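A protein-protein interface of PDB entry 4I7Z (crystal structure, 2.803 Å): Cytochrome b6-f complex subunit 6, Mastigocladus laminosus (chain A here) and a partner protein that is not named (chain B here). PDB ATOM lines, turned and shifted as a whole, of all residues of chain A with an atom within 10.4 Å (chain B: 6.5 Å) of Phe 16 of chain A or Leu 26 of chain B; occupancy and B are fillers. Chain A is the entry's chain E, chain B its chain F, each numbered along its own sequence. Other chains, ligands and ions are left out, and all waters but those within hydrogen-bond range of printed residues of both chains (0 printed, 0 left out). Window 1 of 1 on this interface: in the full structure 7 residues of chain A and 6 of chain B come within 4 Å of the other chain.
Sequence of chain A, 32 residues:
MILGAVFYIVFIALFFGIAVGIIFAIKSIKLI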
ATOM      1  N   TYR A   8      -8.799 -23.832 -18.400  1.00  0.00           N
ATOM      2  CA  TYR A   8      -9.040 -22.998 -17.229  1.00  0.00           C
ATOM      3  C   TYR A   8      -8.254 -21.687 -17.328  1.00  0.00           C
ATOM      4  O   TYR A   8      -8.827 -20.592 -17.217  1.00  0.00           O
ATOM      5  CB  TYR A   8      -8.643 -23.784 -15.976  1.00  0.00           C
ATOM      6  CG  TYR A   8      -8.844 -23.063 -14.667  1.00  0.00           C
ATOM      7  CD1 TYR A   8     -10.103 -22.962 -14.091  1.00  0.00           C
ATOM      8  CD2 TYR A   8      -7.770 -22.506 -13.994  1.00  0.00           C
ATOM      9  CE1 TYR A   8     -10.286 -22.309 -12.888  1.00  0.00           C
ATOM     10  CE2 TYR A   8      -7.939 -21.852 -12.794  1.00  0.00           C
ATOM     11  CZ  TYR A   8      -9.194 -21.759 -12.239  1.00  0.00           C
ATOM     12  OH  TYR A   8      -9.348 -21.098 -11.039  1.00  0.00           O
ATOM     13  N   ILE A   9      -6.945 -21.807 -17.547  1.00  0.00           N
ATOM     14  CA  ILE A   9      -6.080 -20.639 -17.721  1.00  0.00           C
ATOM     15  C   ILE A   9      -6.592 -19.725 -18.835  1.00  0.00           C
ATOM     16  O   ILE A   9      -6.716 -18.521 -18.635  1.00  0.00           O
ATOM     17  CB  ILE A   9      -4.618 -21.043 -18.042  1.00  0.00           C
ATOM     18  CG1 ILE A   9      -3.993 -21.825 -16.886  1.00  0.00           C
ATOM     19  CG2 ILE A   9      -3.768 -19.814 -18.343  1.00  0.00           C
ATOM     20  CD1 ILE A   9      -3.861 -21.043 -15.595  1.00  0.00           C
ATOM     21  N   VAL A  10      -6.881 -20.291 -20.005  1.00  0.00           N
ATOM     22  CA  VAL A  10      -7.365 -19.489 -21.129  1.00  0.00           C
ATOM     23  C   VAL A  10      -8.705 -18.813 -20.808  1.00  0.00           C
ATOM     24  O   VAL A  10      -8.937 -17.667 -21.195  1.00  0.00           O
ATOM     25  CB  VAL A  10      -7.505 -20.342 -22.416  1.00  0.00           C
ATOM     26  CG1 VAL A  10      -8.125 -19.526 -23.555  1.00  0.00           C
ATOM     27  CG2 VAL A  10      -6.147 -20.893 -22.837  1.00  0.00           C
ATOM     28  N   PHE A  11      -9.575 -19.532 -20.104  1.00  0.00           N
ATOM     29  CA  PHE A  11     -10.900 -19.032 -19.725  1.00  0.00           C
ATOM     30  C   PHE A  11     -10.784 -17.823 -18.794  1.00  0.00           C
ATOM     31  O   PHE A  11     -11.290 -16.722 -19.093  1.00  0.00           O
ATOM     32  CB  PHE A  11     -11.676 -20.148 -19.016  1.00  0.00           C
ATOM     33  CG  PHE A  11     -13.159 -20.140 -19.275  1.00  0.00           C
ATOM     34  CD1 PHE A  11     -13.858 -21.337 -19.356  1.00  0.00           C
ATOM     35  CD2 PHE A  11     -13.860 -18.954 -19.407  1.00  0.00           C
ATOM     36  CE1 PHE A  11     -15.221 -21.351 -19.578  1.00  0.00           C
ATOM     37  CE2 PHE A  11     -15.228 -18.963 -19.632  1.00  0.00           C
ATOM     38  CZ  PHE A  11     -15.909 -20.162 -19.717  1.00  0.00           C
ATOM     39  N   ILE A  12     -10.114 -18.027 -17.660  1.00  0.00           N
ATOM     40  CA  ILE A  12      -9.959 -16.948 -16.697  1.00  0.00           C
ATOM     41  C   ILE A  12      -9.144 -15.818 -17.311  1.00  0.00           C
ATOM     42  O   ILE A  12      -9.464 -14.653 -17.114  1.00  0.00           O
ATOM     43  CB  ILE A  12      -9.327 -17.424 -15.373  1.00  0.00           C
ATOM     44  CG1 ILE A  12     -10.255 -18.435 -14.706  1.00  0.00           C
ATOM     45  CG2 ILE A  12      -9.091 -16.241 -14.431  1.00  0.00           C
ATOM     46  CD1 ILE A  12      -9.831 -18.869 -13.326  1.00  0.00           C
ATOM     47  N   ALA A  13      -8.105 -16.159 -18.064  1.00  0.00           N
ATOM     48  CA  ALA A  13      -7.293 -15.140 -18.718  1.00  0.00           C
ATOM     49  C   ALA A  13      -8.167 -14.312 -19.653  1.00  0.00           C
ATOM     50  O   ALA A  13      -8.074 -13.086 -19.676  1.00  0.00           O
ATOM     51  CB  ALA A  13      -6.139 -15.773 -19.483  1.00  0.00           C
ATOM     52  N   LEU A  14      -9.025 -14.989 -20.412  1.00  0.00           N
ATOM     53  CA  LEU A  14      -9.940 -14.311 -21.323  1.00  0.00           C
ATOM     54  C   LEU A  14     -10.826 -13.323 -20.583  1.00  0.00           C
ATOM     55  O   LEU A  14     -10.854 -12.138 -20.917  1.00  0.00           O
ATOM     56  CB  LEU A  14     -10.812 -15.324 -22.064  1.00  0.00           C
ATOM     57  CG  LEU A  14     -10.281 -15.799 -23.412  1.00  0.00           C
ATOM     58  CD1 LEU A  14     -10.996 -17.059 -23.844  1.00  0.00           C
ATOM     59  CD2 LEU A  14     -10.467 -14.708 -24.446  1.00  0.00           C
ATOM     60  N   PHE A  15     -11.547 -13.802 -19.574  1.00  0.00           N
ATOM     61  CA  PHE A  15     -12.454 -12.914 -18.839  1.00  0.00           C
ATOM     62  C   PHE A  15     -11.726 -11.844 -18.007  1.00  0.00           C
ATOM     63  O   PHE A  15     -12.247 -10.746 -17.792  1.00  0.00           O
ATOM     64  CB  PHE A  15     -13.412 -13.727 -17.970  1.00  0.00           C
ATOM     65  CG  PHE A  15     -14.669 -14.130 -18.685  1.00  0.00           C
ATOM     66  CD1 PHE A  15     -14.706 -15.277 -19.455  1.00  0.00           C
ATOM     67  CD2 PHE A  15     -15.808 -13.347 -18.598  1.00  0.00           C
ATOM     68  CE1 PHE A  15     -15.859 -15.641 -20.116  1.00  0.00           C
ATOM     69  CE2 PHE A  15     -16.965 -13.705 -19.258  1.00  0.00           C
ATOM     70  CZ  PHE A  15     -16.992 -14.853 -20.019  1.00  0.00           C
ATOM     71  N   PHE A  16     -10.519 -12.164 -17.558  1.00  0.00           N
ATOM     72  CA  PHE A  16      -9.688 -11.207 -16.842  1.00  0.00           C
ATOM     73  C   PHE A  16      -9.323 -10.092 -17.807  1.00  0.00           C
ATOM     74  O   PHE A  16      -9.423  -8.906 -17.481  1.00  0.00           O
ATOM     75  CB  PHE A  16      -8.423 -11.891 -16.319  1.00  0.00           C
ATOM     76  CG  PHE A  16      -7.583 -11.022 -15.430  1.00  0.00           C
ATOM     77  CD1 PHE A  16      -6.663 -10.136 -15.968  1.00  0.00           C
ATOM     78  CD2 PHE A  16      -7.706 -11.097 -14.054  1.00  0.00           C
ATOM     79  CE1 PHE A  16      -5.887  -9.334 -15.147  1.00  0.00           C
ATOM     80  CE2 PHE A  16      -6.933 -10.300 -13.231  1.00  0.00           C
ATOM     81  CZ  PHE A  16      -6.023  -9.417 -13.778  1.00  0.00           C
ATOM     82  N   GLY A  17      -8.906 -10.491 -19.005  1.00  0.00           N
ATOM     83  CA  GLY A  17      -8.573  -9.553 -20.059  1.00  0.00           C
ATOM     84  C   GLY A  17      -9.764  -8.683 -20.404  1.00  0.00           C
ATOM     85  O   GLY A  17      -9.630  -7.467 -20.547  1.00  0.00           O
ATOM     86  N   ILE A  18     -10.932  -9.308 -20.529  1.00  0.00           N
ATOM     87  CA  ILE A  18     -12.173  -8.568 -20.752  1.00  0.00           C
ATOM     88  C   ILE A  18     -12.403  -7.550 -19.632  1.00  0.00           C
ATOM     89  O   ILE A  18     -12.741  -6.402 -19.902  1.00  0.00           O
ATOM     90  CB  ILE A  18     -13.396  -9.515 -20.877  1.00  0.00           C
ATOM     91  CG1 ILE A  18     -13.280 -10.366 -22.137  1.00  0.00           C
ATOM     92  CG2 ILE A  18     -14.706  -8.727 -20.940  1.00  0.00           C
ATOM     93  CD1 ILE A  18     -14.281 -11.485 -22.199  1.00  0.00           C
ATOM     94  N   ALA A  19     -12.220  -7.961 -18.381  1.00  0.00           N
ATOM     95  CA  ALA A  19     -12.371  -7.035 -17.257  1.00  0.00           C
ATOM     96  C   ALA A  19     -11.416  -5.843 -17.352  1.00  0.00           C
ATOM     97  O   ALA A  19     -11.849  -4.682 -17.389  1.00  0.00           O
ATOM     98  CB  ALA A  19     -12.166  -7.765 -15.940  1.00  0.00           C
ATOM     99  N   VAL A  20     -10.119  -6.135 -17.390  1.00  0.00           N
ATOM    100  CA  VAL A  20      -9.105  -5.090 -17.475  1.00  0.00           C
ATOM    101  C   VAL A  20      -9.326  -4.240 -18.727  1.00  0.00           C
ATOM    102  O   VAL A  20      -9.014  -3.052 -18.743  1.00  0.00           O
ATOM    103  CB  VAL A  20      -7.678  -5.686 -17.477  1.00  0.00           C
ATOM    104  CG1 VAL A  20      -6.624  -4.594 -17.644  1.00  0.00           C
ATOM    105  CG2 VAL A  20      -7.425  -6.468 -16.194  1.00  0.00           C
ATOM    106  N   GLY A  21      -9.878  -4.849 -19.770  1.00  0.00           N
ATOM    107  CA  GLY A  21     -10.197  -4.116 -20.978  1.00  0.00           C
ATOM    108  C   GLY A  21     -11.304  -3.113 -20.724  1.00  0.00           C
ATOM    109  O   GLY A  21     -11.128  -1.909 -20.928  1.00  0.00           O
ATOM    110  N   ILE A  22     -12.447  -3.616 -20.262  1.00  0.00           N
ATOM    111  CA  ILE A  22     -13.628  -2.788 -20.035  1.00  0.00           C
ATOM    112  C   ILE A  22     -13.336  -1.652 -19.054  1.00  0.00           C
ATOM    113  O   ILE A  22     -13.771  -0.523 -19.278  1.00  0.00           O
ATOM    114  CB  ILE A  22     -14.833  -3.620 -19.496  1.00  0.00           C
ATOM    115  CG1 ILE A  22     -15.297  -4.656 -20.523  1.00  0.00           C
ATOM    116  CG2 ILE A  22     -16.005  -2.715 -19.136  1.00  0.00           C
ATOM    117  CD1 ILE A  22     -16.001  -4.081 -21.743  1.00  0.00           C
ATOM    118  N   ILE A  23     -12.616  -1.941 -17.971  1.00  0.00           N
ATOM    119  CA  ILE A  23     -12.338  -0.901 -16.983  1.00  0.00           C
ATOM    120  C   ILE A  23     -11.626   0.295 -17.623  1.00  0.00           C
ATOM    121  O   ILE A  23     -12.042   1.433 -17.435  1.00  0.00           O
ATOM    122  CB  ILE A  23     -11.530  -1.422 -15.765  1.00  0.00           C
ATOM    123  CG1 ILE A  23     -11.227  -0.271 -14.794  1.00  0.00           C
ATOM    124  CG2 ILE A  23     -10.245  -2.084 -16.209  1.00  0.00           C
ATOM    125  CD1 ILE A  23     -10.656  -0.718 -13.464  1.00  0.00           C
ATOM    126  N   PHE A  24     -10.573   0.034 -18.390  1.00  0.00           N
ATOM    127  CA  PHE A  24      -9.814   1.108 -19.022  1.00  0.00           C
ATOM    128  C   PHE A  24     -10.619   1.735 -20.152  1.00  0.00           C
ATOM    129  O   PHE A  24     -10.537   2.941 -20.390  1.00  0.00           O
ATOM    130  CB  PHE A  24      -8.480   0.587 -19.561  1.00  0.00           C
ATOM    131  CG  PHE A  24      -7.506   0.172 -18.489  1.00  0.00           C
ATOM    132  CD1 PHE A  24      -6.632  -0.878 -18.708  1.00  0.00           C
ATOM    133  CD2 PHE A  24      -7.455   0.834 -17.272  1.00  0.00           C
ATOM    134  CE1 PHE A  24      -5.732  -1.266 -17.733  1.00  0.00           C
ATOM    135  CE2 PHE A  24      -6.558   0.450 -16.293  1.00  0.00           C
ATOM    136  CZ  PHE A  24      -5.696  -0.603 -16.525  1.00  0.00           C
ATOM    137  N   LYS A  27     -12.883   3.930 -18.256  1.00  0.00           N
ATOM    138  CA  LYS A  27     -12.136   4.954 -17.523  1.00  0.00           C
ATOM    139  C   LYS A  27     -11.655   6.057 -18.449  1.00  0.00           C
ATOM    140  O   LYS A  27     -12.035   7.217 -18.290  1.00  0.00           O
ATOM    141  CB  LYS A  27     -10.936   4.350 -16.788  1.00  0.00           C
ATOM    142  CG  LYS A  27     -11.061   4.373 -15.271  1.00  0.00           C
ATOM    143  CD  LYS A  27      -9.944   3.588 -14.600  1.00  0.00           C
ATOM    144  CE  LYS A  27     -10.049   3.664 -13.085  1.00  0.00           C
ATOM    145  NZ  LYS A  27      -9.009   2.841 -12.409  1.00  0.00           N
ATOM    146  N   GLY B  21      -6.816 -14.078  -4.948  1.00  0.00           N
ATOM    147  CA  GLY B  21      -5.661 -13.410  -5.517  1.00  0.00           C
ATOM    148  C   GLY B  21      -6.051 -12.598  -6.733  1.00  0.00           C
ATOM    149  O   GLY B  21      -5.582 -11.476  -6.908  1.00  0.00           O
ATOM    150  N   LEU B  22      -6.926 -13.161  -7.562  1.00  0.00           N
ATOM    151  CA  LEU B  22      -7.410 -12.462  -8.749  1.00  0.00           C
ATOM    152  C   LEU B  22      -8.083 -11.147  -8.358  1.00  0.00           C
ATOM    153  O   LEU B  22      -7.740 -10.083  -8.880  1.00  0.00           O
ATOM    154  CB  LEU B  22      -8.391 -13.340  -9.526  1.00  0.00           C
ATOM    155  CG  LEU B  22      -8.470 -13.086 -11.032  1.00  0.00           C
ATOM    156  CD1 LEU B  22      -7.215 -13.608 -11.727  1.00  0.00           C
ATOM    157  CD2 LEU B  22      -9.722 -13.729 -11.611  1.00  0.00           C
ATOM    158  N   GLY B  23      -9.040 -11.226  -7.436  1.00  0.00           N
ATOM    159  CA  GLY B  23      -9.710 -10.040  -6.930  1.00  0.00           C
ATOM    160  C   GLY B  23      -8.720  -8.994  -6.445  1.00  0.00           C
ATOM    161  O   GLY B  23      -8.795  -7.820  -6.829  1.00  0.00           O
ATOM    162  N   VAL B  24      -7.781  -9.423  -5.607  1.00  0.00           N
ATOM    163  CA  VAL B  24      -6.720  -8.535  -5.149  1.00  0.00           C
ATOM    164  C   VAL B  24      -5.966  -7.942  -6.340  1.00  0.00           C
ATOM    165  O   VAL B  24      -5.622  -6.761  -6.342  1.00  0.00           O
ATOM    166  CB  VAL B  24      -5.736  -9.276  -4.223  1.00  0.00           C
ATOM    167  CG1 VAL B  24      -4.572  -8.373  -3.819  1.00  0.00           C
ATOM    168  CG2 VAL B  24      -6.460  -9.779  -2.993  1.00  0.00           C
ATOM    169  N   LEU B  25      -5.721  -8.765  -7.354  1.00  0.00           N
ATOM    170  CA  LEU B  25      -5.005  -8.319  -8.542  1.00  0.00           C
ATOM    171  C   LEU B  25      -5.759  -7.193  -9.248  1.00  0.00           C
ATOM    172  O   LEU B  25      -5.167  -6.174  -9.601  1.00  0.00           O
ATOM    173  CB  LEU B  25      -4.785  -9.484  -9.504  1.00  0.00           C
ATOM    174  CG  LEU B  25      -3.347  -9.666  -9.980  1.00  0.00           C
ATOM    175  CD1 LEU B  25      -3.119 -11.116 -10.354  1.00  0.00           C
ATOM    176  CD2 LEU B  25      -3.059  -8.746 -11.158  1.00  0.00           C
ATOM    177  N   LEU B  26      -7.060  -7.382  -9.464  1.00  0.00           N
ATOM    178  CA  LEU B  26      -7.893  -6.321 -10.033  1.00  0.00           C
ATOM    179  C   LEU B  26      -7.853  -5.056  -9.161  1.00  0.00           C
ATOM    180  O   LEU B  26      -7.721  -3.932  -9.673  1.00  0.00           O
ATOM    181  CB  LEU B  26      -9.348  -6.784 -10.194  1.00  0.00           C
ATOM    182  CG  LEU B  26      -9.753  -7.706 -11.353  1.00  0.00           C
ATOM    183  CD1 LEU B  26      -9.307  -7.159 -12.701  1.00  0.00           C
ATOM    184  CD2 LEU B  26      -9.225  -9.106 -11.147  1.00  0.00           C
ATOM    185  N   LEU B  27      -7.981  -5.240  -7.847  1.00  0.00           N
ATOM    186  CA  LEU B  27      -7.877  -4.122  -6.907  1.00  0.00           C
ATOM    187  C   LEU B  27      -6.572  -3.362  -7.091  1.00  0.00           C
ATOM    188  O   LEU B  27      -6.562  -2.132  -7.100  1.00  0.00           O
ATOM    189  CB  LEU B  27      -7.979  -4.606  -5.462  1.00  0.00           C
ATOM    190  CG  LEU B  27      -9.376  -5.011  -5.000  1.00  0.00           C
ATOM    191  CD1 LEU B  27      -9.305  -5.693  -3.650  1.00  0.00           C
ATOM    192  CD2 LEU B  27     -10.311  -3.814  -4.941  1.00  0.00           C
ATOM    193  N   LYS B  28      -5.472  -4.095  -7.230  1.00  0.00           N
ATOM    194  CA  LYS B  28      -4.172  -3.472  -7.455  1.00  0.00           C
ATOM    195  C   LYS B  28      -4.113  -2.788  -8.816  1.00  0.00           C
ATOM    196  O   LYS B  28      -3.535  -1.710  -8.946  1.00  0.00           O
ATOM    197  CB  LYS B  28      -3.050  -4.501  -7.345  1.00  0.00           C
ATOM    198  CG  LYS B  28      -2.722  -4.903  -5.919  1.00  0.00           C
ATOM    199  CD  LYS B  28      -1.250  -4.676  -5.594  1.00  0.00           C
ATOM    200  CE  LYS B  28      -0.906  -3.191  -5.526  1.00  0.00           C
ATOM    201  NZ  LYS B  28       0.520  -2.947  -5.155  1.00  0.00           N
ATOM    202  N   ILE B  29      -4.707  -3.421  -9.823  1.00  0.00           N
ATOM    203  CA  ILE B  29      -4.725  -2.859 -11.173  1.00  0.00           C
ATOM    204  C   ILE B  29      -5.450  -1.513 -11.213  1.00  0.00           C
ATOM    205  O   ILE B  29      -4.973  -0.577 -11.855  1.00  0.00           O
ATOM    206  CB  ILE B  29      -5.370  -3.831 -12.188  1.00  0.00           C
ATOM    207  CG1 ILE B  29      -4.452  -5.029 -12.431  1.00  0.00           C
ATOM    208  CG2 ILE B  29      -5.639  -3.141 -13.533  1.00  0.00           C
ATOM    209  CD1 ILE B  29      -5.133  -6.200 -13.107  1.00  0.00           C
ATOM    210  N   GLN B  30      -6.591  -1.407 -10.535  1.00  0.00           N
ATOM    211  CA  GLN B  30      -7.319  -0.133 -10.519  1.00  0.00           C
ATOM    212  C   GLN B  30      -6.671   0.875  -9.577  1.00  0.00           C
ATOM    213  O   GLN B  30      -6.690   2.079  -9.830  1.00  0.00           O
ATOM    214  CB  GLN B  30      -8.790  -0.328 -10.138  1.00  0.00           C
ATOM    215  CG  GLN B  30      -9.041  -0.735  -8.687  1.00  0.00           C
ATOM    216  CD  GLN B  30     -10.508  -0.658  -8.311  1.00  0.00           C
ATOM    217  OE1 GLN B  30     -11.374  -0.533  -9.175  1.00  0.00           O
ATOM    218  NE2 GLN B  30     -10.794  -0.732  -7.013  1.00  0.00           N
ATOM    219  N   GLY B  31      -6.102   0.372  -8.486  1.00  0.00           N
ATOM    220  CA  GLY B  31      -5.438   1.212  -7.505  1.00  0.00           C
ATOM    221  C   GLY B  31      -6.387   1.792  -6.468  1.00  0.00           C
ATOM    222  O   GLY B  31      -6.790   2.953  -6.566  1.00  0.00           O
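Of the printed residues of chain B, Phe 16 of chain A touches Leu 22 (3.5 Å), Leu 26 (3.3 Å) and Ile 29 (3.4 Å).
Of the printed residues of chain A, Leu 26 of chain B touches Phe 16 (3.3 Å).
Leu 22 of chain B touches two residues of chain A.
No residue of chain A comes within 4 Å of Gly 23 of chain B.
No residue of chain A comes within 4 Å of Leu 27 of chain B.
Of chain A, only Phe 16, Val 20 and Phe 24 come within 4 Å of Ile 29 of chain B.
Of the printed residues of chain A, Gln 30 of chain B touches Ile 23 and Lys 27.
Printed residues of chain B within 4 Å of Phe 24 of chain A: Ile 29.
Printed residues of chain B within 4 Å of Ile 23 of chain A: Gln 30.
Of the printed residues of chain B, Val 20 of chain A touches Ile 29.
Printed residues of chain B within 4 Å of Lys 27 of chain A: Gln 30 (3.6 Å).
Of the printed residues of chain B, Ile 12 of chain A touches Leu 22.
The nearest printed residue of chain B that does not touch Phe 16 of chain A is Leu 25 of chain B (4.01 Å).
Among the printed residues, pairs that only touch across the chains: Ile 12 of chain A with Leu 22 of chain B, Phe 16 of chain A with Leu 22 of chain B, Phe 16 of chain A with Leu 26 of chain B, Phe 16 of chain A with Ile 29 of chain B, Val 20 of chain A with Ile 29 of chain B, Ile 23 of chain A with Gln 30 of chain B, Phe 24 of chain A with Ile 29 of chain B and Lys 27 of chain A with Gln 30 of chain B.
Printed residues of chain A that touch a printed residue of chain B: Ile 12, Phe 16, Val 20, Ile 23, Phe 24 and Lys 27.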
